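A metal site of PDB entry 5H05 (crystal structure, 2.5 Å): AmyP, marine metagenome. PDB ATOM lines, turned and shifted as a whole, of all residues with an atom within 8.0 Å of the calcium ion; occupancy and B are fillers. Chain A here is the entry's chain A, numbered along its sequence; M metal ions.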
ATOM      1  N   ARG A 301     -22.010 -22.463 -25.104  1.00  0.00           N
ATOM      2  CA  ARG A 301     -21.250 -23.499 -25.797  1.00  0.00           C
ATOM      3  C   ARG A 301     -21.547 -23.495 -27.287  1.00  0.00           C
ATOM      4  O   ARG A 301     -22.670 -23.220 -27.721  1.00  0.00           O
ATOM      5  CB  ARG A 301     -21.560 -24.882 -25.225  1.00  0.00           C
ATOM      6  CG  ARG A 301     -21.003 -25.095 -23.839  1.00  0.00           C
ATOM      7  CD  ARG A 301     -21.029 -26.567 -23.491  1.00  0.00           C
ATOM      8  NE  ARG A 301     -20.507 -26.843 -22.145  1.00  0.00           N
ATOM      9  CZ  ARG A 301     -19.223 -27.002 -21.881  1.00  0.00           C
ATOM     10  NH1 ARG A 301     -18.849 -27.242 -20.633  1.00  0.00           N
ATOM     11  NH2 ARG A 301     -18.324 -26.916 -22.857  1.00  0.00           N
ATOM     12  N   GLY A 303     -21.882 -26.066 -29.202  1.00  0.00           N
ATOM     13  CA  GLY A 303     -22.951 -27.009 -29.476  1.00  0.00           C
ATOM     14  C   GLY A 303     -24.328 -26.412 -29.273  1.00  0.00           C
ATOM     15  O   GLY A 303     -25.236 -26.670 -30.060  1.00  0.00           O
ATOM     16  N   ASP A 304     -24.492 -25.572 -28.249  1.00  0.00           N
ATOM     17  CA  ASP A 304     -25.791 -24.944 -28.027  1.00  0.00           C
ATOM     18  C   ASP A 304     -26.064 -23.788 -29.011  1.00  0.00           C
ATOM     19  O   ASP A 304     -27.224 -23.548 -29.350  1.00  0.00           O
ATOM     20  CB  ASP A 304     -25.872 -24.469 -26.578  1.00  0.00           C
ATOM     21  CG  ASP A 304     -26.088 -25.630 -25.599  1.00  0.00           C
ATOM     22  OD1 ASP A 304     -26.956 -26.496 -25.900  1.00  0.00           O
ATOM     23  OD2 ASP A 304     -25.393 -25.689 -24.551  1.00  0.00           O
ATOM     24  N   LEU A 305     -25.028 -23.083 -29.477  1.00  0.00           N
ATOM     25  CA  LEU A 305     -25.237 -22.107 -30.546  1.00  0.00           C
ATOM     26  C   LEU A 305     -25.695 -22.756 -31.841  1.00  0.00           C
ATOM     27  O   LEU A 305     -26.513 -22.180 -32.575  1.00  0.00           O
ATOM     28  CB  LEU A 305     -23.950 -21.304 -30.794  1.00  0.00           C
ATOM     29  CG  LEU A 305     -23.403 -20.489 -29.620  1.00  0.00           C
ATOM     30  CD1 LEU A 305     -22.068 -19.884 -30.011  1.00  0.00           C
ATOM     31  CD2 LEU A 305     -24.372 -19.401 -29.184  1.00  0.00           C
ATOM     32  N   GLN A 307     -27.537 -25.436 -32.026  1.00  0.00           N
ATOM     33  CA  GLN A 307     -28.935 -25.695 -31.775  1.00  0.00           C
ATOM     34  C   GLN A 307     -29.718 -24.394 -31.671  1.00  0.00           C
ATOM     35  O   GLN A 307     -30.876 -24.320 -32.119  1.00  0.00           O
ATOM     36  CB  GLN A 307     -29.062 -26.519 -30.495  1.00  0.00           C
ATOM     37  CG  GLN A 307     -28.651 -27.954 -30.682  1.00  0.00           C
ATOM     38  CD  GLN A 307     -28.613 -28.711 -29.382  1.00  0.00           C
ATOM     39  OE1 GLN A 307     -29.650 -29.167 -28.881  1.00  0.00           O
ATOM     40  NE2 GLN A 307     -27.410 -28.843 -28.815  1.00  0.00           N
ATOM     41  N   ARG A 308     -29.123 -23.354 -31.085  1.00  0.00           N
ATOM     42  CA  ARG A 308     -29.863 -22.109 -30.940  1.00  0.00           C
ATOM     43  C   ARG A 308     -30.273 -21.578 -32.300  1.00  0.00           C
ATOM     44  O   ARG A 308     -31.446 -21.245 -32.521  1.00  0.00           O
ATOM     45  CB  ARG A 308     -29.042 -21.065 -30.185  1.00  0.00           C
ATOM     46  CG  ARG A 308     -29.755 -19.724 -30.111  1.00  0.00           C
ATOM     47  CD  ARG A 308     -28.999 -18.740 -29.256  1.00  0.00           C
ATOM     48  NE  ARG A 308     -29.017 -19.131 -27.847  1.00  0.00           N
ATOM     49  CZ  ARG A 308     -28.569 -18.354 -26.871  1.00  0.00           C
ATOM     50  NH1 ARG A 308     -28.625 -18.784 -25.629  1.00  0.00           N
ATOM     51  NH2 ARG A 308     -28.074 -17.163 -27.139  1.00  0.00           N
ATOM     52  N   SER A 313     -27.831 -30.390 -34.819  1.00  0.00           N
ATOM     53  CA  SER A 313     -28.109 -31.011 -33.528  1.00  0.00           C
ATOM     54  C   SER A 313     -27.236 -32.248 -33.396  1.00  0.00           C
ATOM     55  O   SER A 313     -26.814 -32.821 -34.406  1.00  0.00           O
ATOM     56  CB  SER A 313     -29.594 -31.371 -33.422  1.00  0.00           C
ATOM     57  OG  SER A 313     -30.072 -31.111 -32.113  1.00  0.00           O
ATOM     58  N   PRO A 314     -26.942 -32.679 -32.171  1.00  0.00           N
ATOM     59  CA  PRO A 314     -25.980 -33.777 -31.977  1.00  0.00           C
ATOM     60  C   PRO A 314     -26.288 -35.066 -32.726  1.00  0.00           C
ATOM     61  O   PRO A 314     -25.368 -35.855 -32.977  1.00  0.00           O
ATOM     62  CB  PRO A 314     -26.016 -33.987 -30.466  1.00  0.00           C
ATOM     63  CG  PRO A 314     -26.398 -32.660 -29.914  1.00  0.00           C
ATOM     64  CD  PRO A 314     -27.361 -32.077 -30.897  1.00  0.00           C
ATOM     65  N   TYR A 319     -23.537 -31.188 -37.211  1.00  0.00           N
ATOM     66  CA  TYR A 319     -23.160 -30.722 -35.874  1.00  0.00           C
ATOM     67  C   TYR A 319     -21.719 -31.105 -35.550  1.00  0.00           C
ATOM     68  O   TYR A 319     -20.970 -30.300 -34.976  1.00  0.00           O
ATOM     69  CB  TYR A 319     -24.132 -31.305 -34.845  1.00  0.00           C
ATOM     70  CG  TYR A 319     -23.850 -31.055 -33.376  1.00  0.00           C
ATOM     71  CD1 TYR A 319     -22.919 -31.818 -32.682  1.00  0.00           C
ATOM     72  CD2 TYR A 319     -24.568 -30.099 -32.672  1.00  0.00           C
ATOM     73  CE1 TYR A 319     -22.675 -31.597 -31.345  1.00  0.00           C
ATOM     74  CE2 TYR A 319     -24.339 -29.896 -31.330  1.00  0.00           C
ATOM     75  CZ  TYR A 319     -23.404 -30.646 -30.670  1.00  0.00           C
ATOM     76  OH  TYR A 319     -23.161 -30.436 -29.340  1.00  0.00           O
ATOM     77  N   ASP A 347     -19.806 -30.895 -26.295  1.00  0.00           N
ATOM     78  CA  ASP A 347     -20.768 -30.870 -25.196  1.00  0.00           C
ATOM     79  C   ASP A 347     -21.841 -29.832 -25.414  1.00  0.00           C
ATOM     80  O   ASP A 347     -21.631 -28.788 -26.038  1.00  0.00           O
ATOM     81  CB  ASP A 347     -20.037 -30.574 -23.892  1.00  0.00           C
ATOM     82  CG  ASP A 347     -20.420 -31.522 -22.789  1.00  0.00           C
ATOM     83  OD1 ASP A 347     -21.470 -32.196 -22.932  1.00  0.00           O
ATOM     84  OD2 ASP A 347     -19.658 -31.577 -21.794  1.00  0.00           O
ATOM     85  N   GLU A 348     -23.022 -30.118 -24.882  1.00  0.00           N
ATOM     86  CA  GLU A 348     -24.108 -29.161 -24.900  1.00  0.00           C
ATOM     87  C   GLU A 348     -25.052 -29.516 -23.757  1.00  0.00           C
ATOM     88  O   GLU A 348     -25.045 -30.655 -23.261  1.00  0.00           O
ATOM     89  CB  GLU A 348     -24.824 -29.150 -26.256  1.00  0.00           C
ATOM     90  CG  GLU A 348     -25.170 -30.534 -26.807  1.00  0.00           C
ATOM     91  CD  GLU A 348     -26.462 -31.109 -26.234  1.00  0.00           C
ATOM     92  OE1 GLU A 348     -27.533 -30.471 -26.389  1.00  0.00           O
ATOM     93  OE2 GLU A 348     -26.410 -32.204 -25.619  1.00  0.00           O
ATOM     94  N   LEU A 349     -25.853 -28.540 -23.340  1.00  0.00           N
ATOM     95  CA  LEU A 349     -26.762 -28.704 -22.220  1.00  0.00           C
ATOM     96  C   LEU A 349     -28.079 -29.264 -22.719  1.00  0.00           C
ATOM     97  O   LEU A 349     -28.839 -28.567 -23.386  1.00  0.00           O
ATOM     98  CB  LEU A 349     -26.988 -27.377 -21.511  1.00  0.00           C
ATOM     99  CG  LEU A 349     -28.002 -27.381 -20.374  1.00  0.00           C
ATOM    100  CD1 LEU A 349     -27.717 -28.484 -19.393  1.00  0.00           C
ATOM    101  CD2 LEU A 349     -27.980 -26.032 -19.679  1.00  0.00           C
ATOM    102  N   GLU A 350     -28.365 -30.525 -22.372  1.00  0.00           N
ATOM    103  CA  GLU A 350     -29.588 -31.171 -22.843  1.00  0.00           C
ATOM    104  C   GLU A 350     -30.815 -30.359 -22.457  1.00  0.00           C
ATOM    105  O   GLU A 350     -30.967 -29.915 -21.312  1.00  0.00           O
ATOM    106  CB  GLU A 350     -29.687 -32.586 -22.290  1.00  0.00           C
ATOM    107  CG  GLU A 350     -31.029 -33.257 -22.526  1.00  0.00           C
ATOM    108  CD  GLU A 350     -30.923 -34.774 -22.486  1.00  0.00           C
ATOM    109  OE1 GLU A 350     -30.121 -35.339 -23.277  1.00  0.00           O
ATOM    110  OE2 GLU A 350     -31.640 -35.406 -21.673  1.00  0.00           O
ATOM    111  N   GLY A 351     -31.697 -30.131 -23.427  1.00  0.00           N
ATOM    112  CA  GLY A 351     -32.917 -29.404 -23.146  1.00  0.00           C
ATOM    113  C   GLY A 351     -32.787 -27.906 -23.174  1.00  0.00           C
ATOM    114  O   GLY A 351     -33.746 -27.210 -22.817  1.00  0.00           O
ATOM    115  N   TYR A 352     -31.642 -27.382 -23.574  1.00  0.00           N
ATOM    116  CA  TYR A 352     -31.409 -25.953 -23.615  1.00  0.00           C
ATOM    117  C   TYR A 352     -30.913 -25.552 -24.999  1.00  0.00           C
ATOM    118  O   TYR A 352     -30.077 -26.241 -25.582  1.00  0.00           O
ATOM    119  CB  TYR A 352     -30.371 -25.573 -22.567  1.00  0.00           C
ATOM    120  CG  TYR A 352     -29.827 -24.186 -22.765  1.00  0.00           C
ATOM    121  CD1 TYR A 352     -28.671 -23.955 -23.506  1.00  0.00           C
ATOM    122  CD2 TYR A 352     -30.480 -23.089 -22.205  1.00  0.00           C
ATOM    123  CE1 TYR A 352     -28.184 -22.691 -23.678  1.00  0.00           C
ATOM    124  CE2 TYR A 352     -30.005 -21.831 -22.378  1.00  0.00           C
ATOM    125  CZ  TYR A 352     -28.851 -21.612 -23.113  1.00  0.00           C
ATOM    126  OH  TYR A 352     -28.391 -20.329 -23.272  1.00  0.00           O
ATOM    127  N   ALA A 353     -31.387 -24.429 -25.499  1.00  0.00           N
ATOM    128  CA  ALA A 353     -30.801 -23.880 -26.721  1.00  0.00           C
ATOM    129  C   ALA A 353     -31.128 -22.403 -26.839  1.00  0.00           C
ATOM    130  O   ALA A 353     -30.236 -21.549 -26.857  1.00  0.00           O
ATOM    131  CB  ALA A 353     -31.282 -24.646 -27.953  1.00  0.00           C
ATOM    132  N   GLN A 354     -32.422 -22.095 -26.904  1.00  0.00           N
ATOM    133  CA  GLN A 354     -32.860 -20.712 -27.005  1.00  0.00           C
ATOM    134  C   GLN A 354     -32.417 -19.922 -25.781  1.00  0.00           C
ATOM    135  O   GLN A 354     -32.310 -20.453 -24.663  1.00  0.00           O
ATOM    136  CB  GLN A 354     -34.377 -20.661 -27.167  1.00  0.00           C
ATOM    137  CG  GLN A 354     -34.869 -21.167 -28.506  1.00  0.00           C
ATOM    138  CD  GLN A 354     -34.696 -20.129 -29.615  1.00  0.00           C
ATOM    139  OE1 GLN A 354     -33.621 -20.036 -30.227  1.00  0.00           O
ATOM    140  NE2 GLN A 354     -35.749 -19.330 -29.874  1.00  0.00           N
HETATM  141 CA    CA M   1     -28.717 -28.249 -25.851  1.00  0.00          CA
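NH1 of Arg 308 lies within hydrogen-bond range of OH of Tyr 352 (2.8 Å).
OE1 of Glu 348 sits close to NE2 of Gln 307 (2.9 Å).
NE2 of Gln 307 sits at hydrogen-bond distance from O of Gly 303 (3.3 Å).
Gln 307 touches the calcium ion.
Five residues have an atom within 4 Å of the calcium ion: Asp 304, Gln 307, Glu 348, Leu 349 and Tyr 352.
Along chain A the residues within 4 Å of the calcium ion span positions 304 to 352.
The calcium ion is bound by the backbone carbonyl oxygen (O) of Tyr 352 (2.4 Å), the side-chain carboxylate (OD1) of Asp 304 (2.5 Å), the backbone carbonyl oxygen (O) of Leu 349 (2.5 Å) and the side-chain carboxylate (OE1) of Glu 348 (2.6 Å).
The calcium ion has four donor atoms within binding distance.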
